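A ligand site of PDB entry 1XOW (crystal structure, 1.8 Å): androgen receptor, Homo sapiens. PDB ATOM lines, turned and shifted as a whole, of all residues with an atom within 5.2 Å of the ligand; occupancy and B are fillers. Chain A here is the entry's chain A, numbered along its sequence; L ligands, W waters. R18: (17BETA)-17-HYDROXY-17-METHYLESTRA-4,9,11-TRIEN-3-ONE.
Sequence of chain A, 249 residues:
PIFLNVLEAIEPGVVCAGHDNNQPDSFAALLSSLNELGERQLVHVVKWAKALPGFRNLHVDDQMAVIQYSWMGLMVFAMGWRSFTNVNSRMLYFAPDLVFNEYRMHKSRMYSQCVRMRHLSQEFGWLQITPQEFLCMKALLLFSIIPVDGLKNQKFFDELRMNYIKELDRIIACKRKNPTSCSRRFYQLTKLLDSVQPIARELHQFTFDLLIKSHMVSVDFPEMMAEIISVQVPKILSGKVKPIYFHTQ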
ATOM      1  N   LEU A  31      10.077  -6.164  13.923  1.00  0.00           N
ATOM      2  CA  LEU A  31      10.018  -5.889  15.352  1.00  0.00           C
ATOM      3  C   LEU A  31       8.940  -6.701  16.048  1.00  0.00           C
ATOM      4  O   LEU A  31       9.116  -7.130  17.182  1.00  0.00           O
ATOM      5  CB  LEU A  31       9.848  -4.392  15.594  1.00  0.00           C
ATOM      6  CG  LEU A  31      11.104  -3.583  15.248  1.00  0.00           C
ATOM      7  CD1 LEU A  31      10.855  -2.148  15.590  1.00  0.00           C
ATOM      8  CD2 LEU A  31      12.307  -4.100  16.029  1.00  0.00           C
ATOM      9  N   LEU A  34      10.307 -10.056  16.533  1.00  0.00           N
ATOM     10  CA  LEU A  34      11.290 -10.048  17.610  1.00  0.00           C
ATOM     11  C   LEU A  34      10.581 -10.065  18.965  1.00  0.00           C
ATOM     12  O   LEU A  34      10.998 -10.757  19.892  1.00  0.00           O
ATOM     13  CB  LEU A  34      12.180  -8.799  17.520  1.00  0.00           C
ATOM     14  CG  LEU A  34      13.400  -8.894  16.599  1.00  0.00           C
ATOM     15  CD1 LEU A  34      14.087  -7.541  16.517  1.00  0.00           C
ATOM     16  CD2 LEU A  34      14.362  -9.951  17.121  1.00  0.00           C
ATOM     17  N   ASN A  35       9.485  -9.310  19.064  1.00  0.00           N
ATOM     18  CA  ASN A  35       8.735  -9.268  20.309  1.00  0.00           C
ATOM     19  C   ASN A  35       8.157 -10.646  20.642  1.00  0.00           C
ATOM     20  O   ASN A  35       8.143 -11.061  21.804  1.00  0.00           O
ATOM     21  CB  ASN A  35       7.631  -8.224  20.247  1.00  0.00           C
ATOM     22  CG  ASN A  35       8.154  -6.815  20.374  1.00  0.00           C
ATOM     23  OD1 ASN A  35       9.244  -6.607  20.900  1.00  0.00           O
ATOM     24  ND2 ASN A  35       7.375  -5.833  19.914  1.00  0.00           N
ATOM     25  N   LEU A  37       9.387 -13.482  19.673  1.00  0.00           N
ATOM     26  CA  LEU A  37      10.542 -14.303  20.025  1.00  0.00           C
ATOM     27  C   LEU A  37      10.924 -14.023  21.476  1.00  0.00           C
ATOM     28  O   LEU A  37      11.249 -14.930  22.233  1.00  0.00           O
ATOM     29  CB  LEU A  37      11.728 -13.969  19.102  1.00  0.00           C
ATOM     30  CG  LEU A  37      13.022 -14.736  19.414  1.00  0.00           C
ATOM     31  CD1 LEU A  37      12.761 -16.235  19.329  1.00  0.00           C
ATOM     32  CD2 LEU A  37      14.126 -14.324  18.450  1.00  0.00           C
ATOM     33  N   GLY A  38      10.899 -12.742  21.850  1.00  0.00           N
ATOM     34  CA  GLY A  38      11.238 -12.354  23.201  1.00  0.00           C
ATOM     35  C   GLY A  38      10.322 -13.009  24.208  1.00  0.00           C
ATOM     36  O   GLY A  38      10.790 -13.469  25.243  1.00  0.00           O
ATOM     37  N   GLN A  41      11.241 -16.660  24.391  1.00  0.00           N
ATOM     38  CA  GLN A  41      12.493 -16.856  25.121  1.00  0.00           C
ATOM     39  C   GLN A  41      12.324 -16.574  26.598  1.00  0.00           C
ATOM     40  O   GLN A  41      13.028 -17.157  27.416  1.00  0.00           O
ATOM     41  CB  GLN A  41      13.608 -15.972  24.544  1.00  0.00           C
ATOM     42  CG  GLN A  41      14.083 -16.423  23.169  1.00  0.00           C
ATOM     43  CD  GLN A  41      15.427 -15.831  22.766  1.00  0.00           C
ATOM     44  OE1 GLN A  41      15.902 -16.051  21.650  1.00  0.00           O
ATOM     45  NE2 GLN A  41      16.047 -15.086  23.667  1.00  0.00           N
ATOM     46  N   TRP A  71      16.380 -10.171  32.136  1.00  0.00           N
ATOM     47  CA  TRP A  71      15.825 -10.695  30.895  1.00  0.00           C
ATOM     48  C   TRP A  71      16.528 -10.208  29.617  1.00  0.00           C
ATOM     49  O   TRP A  71      16.970 -11.008  28.794  1.00  0.00           O
ATOM     50  CB  TRP A  71      14.314 -10.395  30.863  1.00  0.00           C
ATOM     51  CG  TRP A  71      13.616 -10.494  29.519  1.00  0.00           C
ATOM     52  CD1 TRP A  71      13.437 -11.594  28.752  1.00  0.00           C
ATOM     53  CD2 TRP A  71      12.955  -9.408  28.849  1.00  0.00           C
ATOM     54  NE1 TRP A  71      12.703 -11.244  27.616  1.00  0.00           N
ATOM     55  CE2 TRP A  71      12.399  -9.913  27.657  1.00  0.00           C
ATOM     56  CE3 TRP A  71      12.798  -8.031  29.151  1.00  0.00           C
ATOM     57  CZ2 TRP A  71      11.679  -9.120  26.759  1.00  0.00           C
ATOM     58  CZ3 TRP A  71      12.087  -7.228  28.243  1.00  0.00           C
ATOM     59  CH2 TRP A  71      11.533  -7.793  27.052  1.00  0.00           C
ATOM     60  N   MET A  72      16.626  -8.895  29.462  1.00  0.00           N
ATOM     61  CA  MET A  72      17.256  -8.320  28.283  1.00  0.00           C
ATOM     62  C   MET A  72      18.721  -8.733  28.115  1.00  0.00           C
ATOM     63  O   MET A  72      19.123  -9.196  27.040  1.00  0.00           O
ATOM     64  CB  MET A  72      17.155  -6.792  28.335  1.00  0.00           C
ATOM     65  CG  MET A  72      17.632  -6.103  27.035  1.00  0.00           C
ATOM     66  SD  MET A  72      16.563  -6.495  25.650  1.00  0.00           S
ATOM     67  CE  MET A  72      15.127  -5.489  26.075  1.00  0.00           C
ATOM     68  N   MET A  75      19.157 -12.396  27.165  1.00  0.00           N
ATOM     69  CA  MET A  75      18.855 -12.653  25.764  1.00  0.00           C
ATOM     70  C   MET A  75      19.966 -12.171  24.850  1.00  0.00           C
ATOM     71  O   MET A  75      20.345 -12.863  23.905  1.00  0.00           O
ATOM     72  CB  MET A  75      17.535 -11.987  25.362  1.00  0.00           C
ATOM     73  CG  MET A  75      16.298 -12.555  26.046  1.00  0.00           C
ATOM     74  SD  MET A  75      14.786 -12.038  25.194  1.00  0.00           S
ATOM     75  CE  MET A  75      14.898 -10.263  25.306  1.00  0.00           C
ATOM     76  N   VAL A  76      20.485 -10.982  25.148  1.00  0.00           N
ATOM     77  CA  VAL A  76      21.562 -10.400  24.362  1.00  0.00           C
ATOM     78  C   VAL A  76      22.801 -11.280  24.385  1.00  0.00           C
ATOM     79  O   VAL A  76      23.398 -11.566  23.350  1.00  0.00           O
ATOM     80  CB  VAL A  76      21.933  -8.994  24.918  1.00  0.00           C
ATOM     81  CG1 VAL A  76      23.252  -8.524  24.335  1.00  0.00           C
ATOM     82  CG2 VAL A  76      20.822  -8.002  24.606  1.00  0.00           C
ATOM     83  N   MET A  79      22.211 -14.580  22.546  1.00  0.00           N
ATOM     84  CA  MET A  79      22.102 -14.311  21.114  1.00  0.00           C
ATOM     85  C   MET A  79      23.510 -14.107  20.543  1.00  0.00           C
ATOM     86  O   MET A  79      23.834 -14.622  19.467  1.00  0.00           O
ATOM     87  CB  MET A  79      21.232 -13.069  20.892  1.00  0.00           C
ATOM     88  CG  MET A  79      20.853 -12.799  19.438  1.00  0.00           C
ATOM     89  SD  MET A  79      22.121 -11.911  18.513  1.00  0.00           S
ATOM     90  CE  MET A  79      21.902 -10.254  19.194  1.00  0.00           C
ATOM     91  N   ARG A  82      25.082 -17.440  20.179  1.00  0.00           N
ATOM     92  CA  ARG A  82      24.513 -18.154  19.039  1.00  0.00           C
ATOM     93  C   ARG A  82      25.054 -17.623  17.720  1.00  0.00           C
ATOM     94  O   ARG A  82      25.316 -18.389  16.785  1.00  0.00           O
ATOM     95  CB  ARG A  82      22.978 -18.024  19.028  1.00  0.00           C
ATOM     96  CG  ARG A  82      22.267 -18.843  20.097  1.00  0.00           C
ATOM     97  CD  ARG A  82      20.794 -19.003  19.737  1.00  0.00           C
ATOM     98  NE  ARG A  82      20.102 -17.725  19.637  1.00  0.00           N
ATOM     99  CZ  ARG A  82      19.711 -17.002  20.681  1.00  0.00           C
ATOM    100  NH1 ARG A  82      19.927 -17.429  21.924  1.00  0.00           N
ATOM    101  NH2 ARG A  82      19.094 -15.843  20.491  1.00  0.00           N
ATOM    102  N   PHE A  94      19.243 -14.240  15.854  1.00  0.00           N
ATOM    103  CA  PHE A  94      18.202 -14.139  16.877  1.00  0.00           C
ATOM    104  C   PHE A  94      17.505 -15.501  17.018  1.00  0.00           C
ATOM    105  O   PHE A  94      17.192 -15.936  18.118  1.00  0.00           O
ATOM    106  CB  PHE A  94      17.179 -13.063  16.495  1.00  0.00           C
ATOM    107  CG  PHE A  94      17.683 -11.665  16.671  1.00  0.00           C
ATOM    108  CD1 PHE A  94      17.928 -11.161  17.951  1.00  0.00           C
ATOM    109  CD2 PHE A  94      17.944 -10.862  15.569  1.00  0.00           C
ATOM    110  CE1 PHE A  94      18.425  -9.873  18.128  1.00  0.00           C
ATOM    111  CE2 PHE A  94      18.441  -9.574  15.737  1.00  0.00           C
ATOM    112  CZ  PHE A  94      18.686  -9.079  17.006  1.00  0.00           C
ATOM    113  N   MET A 110      17.121  -0.419  14.245  1.00  0.00           N
ATOM    114  CA  MET A 110      17.855  -0.790  15.451  1.00  0.00           C
ATOM    115  C   MET A 110      19.325  -0.974  15.082  1.00  0.00           C
ATOM    116  O   MET A 110      20.072  -1.626  15.800  1.00  0.00           O
ATOM    117  CB  MET A 110      17.365  -2.124  16.004  1.00  0.00           C
ATOM    118  CG  MET A 110      16.494  -2.036  17.228  1.00  0.00           C
ATOM    119  SD  MET A 110      16.429  -3.605  18.125  1.00  0.00           S
ATOM    120  CE  MET A 110      15.640  -4.647  16.974  1.00  0.00           C
ATOM    121  N   MET A 117      25.558  -5.260  19.565  1.00  0.00           N
ATOM    122  CA  MET A 117      25.353  -6.677  19.810  1.00  0.00           C
ATOM    123  C   MET A 117      26.267  -7.532  18.941  1.00  0.00           C
ATOM    124  O   MET A 117      26.739  -8.585  19.369  1.00  0.00           O
ATOM    125  CB  MET A 117      23.886  -7.056  19.542  1.00  0.00           C
ATOM    126  CG  MET A 117      22.920  -6.472  20.563  1.00  0.00           C
ATOM    127  SD  MET A 117      21.219  -7.059  20.404  1.00  0.00           S
ATOM    128  CE  MET A 117      20.623  -6.004  19.135  1.00  0.00           C
ATOM    129  N   LEU A 203      18.968  -1.198  24.691  1.00  0.00           N
ATOM    130  CA  LEU A 203      17.825  -1.968  24.237  1.00  0.00           C
ATOM    131  C   LEU A 203      16.610  -1.703  25.127  1.00  0.00           C
ATOM    132  O   LEU A 203      15.483  -1.712  24.660  1.00  0.00           O
ATOM    133  CB  LEU A 203      18.174  -3.458  24.226  1.00  0.00           C
ATOM    134  CG  LEU A 203      19.223  -3.809  23.155  1.00  0.00           C
ATOM    135  CD1 LEU A 203      19.738  -5.212  23.395  1.00  0.00           C
ATOM    136  CD2 LEU A 203      18.599  -3.706  21.760  1.00  0.00           C
ATOM    137  N   PHE A 206      15.212   1.507  23.933  1.00  0.00           N
ATOM    138  CA  PHE A 206      14.597   1.300  22.640  1.00  0.00           C
ATOM    139  C   PHE A 206      13.260   0.557  22.734  1.00  0.00           C
ATOM    140  O   PHE A 206      12.280   0.972  22.135  1.00  0.00           O
ATOM    141  CB  PHE A 206      15.569   0.537  21.710  1.00  0.00           C
ATOM    142  CG  PHE A 206      15.026   0.283  20.327  1.00  0.00           C
ATOM    143  CD1 PHE A 206      14.244  -0.825  20.077  1.00  0.00           C
ATOM    144  CD2 PHE A 206      15.284   1.176  19.285  1.00  0.00           C
ATOM    145  CE1 PHE A 206      13.720  -1.068  18.805  1.00  0.00           C
ATOM    146  CE2 PHE A 206      14.769   0.963  18.002  1.00  0.00           C
ATOM    147  CZ  PHE A 206      13.978  -0.185  17.762  1.00  0.00           C
ATOM    148  N   THR A 207      13.231  -0.541  23.479  1.00  0.00           N
ATOM    149  CA  THR A 207      11.995  -1.301  23.604  1.00  0.00           C
ATOM    150  C   THR A 207      10.923  -0.502  24.363  1.00  0.00           C
ATOM    151  O   THR A 207       9.738  -0.612  24.075  1.00  0.00           O
ATOM    152  CB  THR A 207      12.226  -2.691  24.282  1.00  0.00           C
ATOM    153  OG1 THR A 207      11.104  -3.539  24.028  1.00  0.00           O
ATOM    154  CG2 THR A 207      12.401  -2.538  25.783  1.00  0.00           C
ATOM    155  N   LEU A 210       9.534   2.053  22.011  1.00  0.00           N
ATOM    156  CA  LEU A 210       8.765   1.312  21.010  1.00  0.00           C
ATOM    157  C   LEU A 210       7.382   0.939  21.562  1.00  0.00           C
ATOM    158  O   LEU A 210       6.374   1.023  20.855  1.00  0.00           O
ATOM    159  CB  LEU A 210       9.529   0.054  20.591  1.00  0.00           C
ATOM    160  CG  LEU A 210       8.936  -0.851  19.501  1.00  0.00           C
ATOM    161  CD1 LEU A 210       8.657  -0.046  18.245  1.00  0.00           C
ATOM    162  CD2 LEU A 210       9.905  -1.981  19.213  1.00  0.00           C
ATOM    163  N   PHE A 221       3.024  -6.080  20.835  1.00  0.00           N
ATOM    164  CA  PHE A 221       3.741  -6.521  22.032  1.00  0.00           C
ATOM    165  C   PHE A 221       2.941  -7.594  22.772  1.00  0.00           C
ATOM    166  O   PHE A 221       1.780  -7.370  23.143  1.00  0.00           O
ATOM    167  CB  PHE A 221       3.997  -5.357  22.998  1.00  0.00           C
ATOM    168  CG  PHE A 221       5.172  -4.500  22.632  1.00  0.00           C
ATOM    169  CD1 PHE A 221       5.067  -3.548  21.627  1.00  0.00           C
ATOM    170  CD2 PHE A 221       6.383  -4.648  23.291  1.00  0.00           C
ATOM    171  CE1 PHE A 221       6.154  -2.734  21.291  1.00  0.00           C
ATOM    172  CE2 PHE A 221       7.479  -3.843  22.965  1.00  0.00           C
ATOM    173  CZ  PHE A 221       7.365  -2.891  21.970  1.00  0.00           C
ATOM    174  N   MET A 225       5.500  -9.206  27.947  1.00  0.00           N
ATOM    175  CA  MET A 225       6.471  -8.206  27.549  1.00  0.00           C
ATOM    176  C   MET A 225       5.983  -6.799  27.839  1.00  0.00           C
ATOM    177  O   MET A 225       6.702  -5.983  28.410  1.00  0.00           O
ATOM    178  CB  MET A 225       6.785  -8.343  26.072  1.00  0.00           C
ATOM    179  CG  MET A 225       7.382  -9.676  25.692  1.00  0.00           C
ATOM    180  SD  MET A 225       8.980  -9.457  24.942  1.00  0.00           S
ATOM    181  CE  MET A 225       8.660  -8.012  23.903  1.00  0.00           C
ATOM    182  N   ILE A 229       7.911  -4.483  30.411  1.00  0.00           N
ATOM    183  CA  ILE A 229       8.505  -3.265  29.870  1.00  0.00           C
ATOM    184  C   ILE A 229       7.889  -2.002  30.469  1.00  0.00           C
ATOM    185  O   ILE A 229       8.566  -0.979  30.569  1.00  0.00           O
ATOM    186  CB  ILE A 229       8.374  -3.227  28.328  1.00  0.00           C
ATOM    187  CG1 ILE A 229       9.157  -4.405  27.729  1.00  0.00           C
ATOM    188  CG2 ILE A 229       8.895  -1.902  27.776  1.00  0.00           C
ATOM    189  CD1 ILE A 229       9.002  -4.568  26.209  1.00  0.00           C
HETATM  190  C1  R18 L   1      14.766 -11.499  21.091  1.00  0.00           C
HETATM  191  C2  R18 L   1      15.622 -12.679  21.522  1.00  0.00           C
HETATM  192  C3  R18 L   1      17.108 -12.501  21.362  1.00  0.00           C
HETATM  193  C4  R18 L   1      17.623 -11.182  21.699  1.00  0.00           C
HETATM  194  C5  R18 L   1      16.855 -10.046  21.758  1.00  0.00           C
HETATM  195  C6  R18 L   1      17.509  -8.682  22.136  1.00  0.00           C
HETATM  196  C7  R18 L   1      16.726  -7.551  21.446  1.00  0.00           C
HETATM  197  C8  R18 L   1      15.243  -7.577  21.866  1.00  0.00           C
HETATM  198  C9  R18 L   1      14.610  -8.970  21.518  1.00  0.00           C
HETATM  199  C10 R18 L   1      15.368 -10.086  21.448  1.00  0.00           C
HETATM  200  C11 R18 L   1      13.141  -8.969  21.298  1.00  0.00           C
HETATM  201  C12 R18 L   1      12.364  -7.864  21.367  1.00  0.00           C
HETATM  202  C13 R18 L   1      12.917  -6.483  21.655  1.00  0.00           C
HETATM  203  C14 R18 L   1      14.410  -6.437  21.195  1.00  0.00           C
HETATM  204  C15 R18 L   1      14.890  -4.979  21.491  1.00  0.00           C
HETATM  205  C16 R18 L   1      13.557  -4.234  21.188  1.00  0.00           C
HETATM  206  C17 R18 L   1      12.403  -5.274  20.855  1.00  0.00           C
HETATM  207  C18 R18 L   1      12.839  -6.248  23.223  1.00  0.00           C
HETATM  208  C27 R18 L   1      12.369  -5.452  19.356  1.00  0.00           C
HETATM  209  O83 R18 L   1      17.851 -13.419  21.041  1.00  0.00           O
HETATM  210  O97 R18 L   1      11.181  -4.720  21.384  1.00  0.00           O
HETATM  211  O   HOH W   1      18.761 -15.099  23.385  1.00  0.00           O
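An oxygen (O97) of the ligand lies within hydrogen-bond range of the side-chain hydroxyl (OG1) of Thr 207, 2.9 Å away.
The guanidinium group (NH2) of Arg 82 sits at hydrogen-bond distance from an oxygen (O83) of the ligand, 2.8 Å away.
An oxygen (O97) of the ligand sits at hydrogen-bond distance from the side-chain amide oxygen (OD1) of Asn 35.
OE1 of Gln 41 sits close to O83 of the ligand.
NH2 of Arg 82 sits at hydrogen-bond distance from O of Phe 94.
The side-chain amide nitrogen of Asn 35 lies close to the backbone carbonyl oxygen of Leu 31, 3.5 Å away.
NE2 of Gln 41 sits close to SD of Met 75 (3.6 Å).
The guanidinium group (NH2) of Arg 82 sits at hydrogen-bond distance from the side-chain amide oxygen (OE1) of Gln 41 (3.4 Å).
The side-chain sulfur (SD) of Met 75 is in hydrogen-bond range of the indole nitrogen (NE1) of Trp 71.
CD2 of Leu 31 touches C27 of the ligand, 3.6 Å away.
Leu 34 touches the ligand.
Leu 37 touches the ligand (CD2 to C2, 3.8 Å).
Met 72 touches the ligand.
Met 75 touches the ligand.
Met 79 touches the ligand.
Phe 94 touches the ligand (CD1 to C3, 3.8 Å).
Met 110 touches the ligand (SD to C15, 3.9 Å).
Leu 203 touches the ligand (CD2 to C15, 3.9 Å).
Phe 206 touches the ligand (CD1 to C16, 3.7 Å).
CD2 of Leu 210 touches O97 of the ligand, at 3.7 Å.
Hydrophobic or aromatic side chains that line the ligand: Leu 31, Leu 34, Leu 37, Met 72, Met 75, Met 79, Phe 94, Met 110, Leu 203, Phe 206 and Leu 210.
Within 4 Å of the ligand: Leu 31, Leu 34, Asn 35, Leu 37, Gln 41, Met 72, Met 75, Met 79, Arg 82, Phe 94, Met 110, Leu 203, Phe 206, Thr 207 and Leu 210.
Water W1 lies within hydrogen-bond range of NE2 of Gln 41 (2.7 Å), O of Met 75 (2.8 Å), NH1 of Arg 82 (3.0 Å) and O83 of the ligand (3.0 Å).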
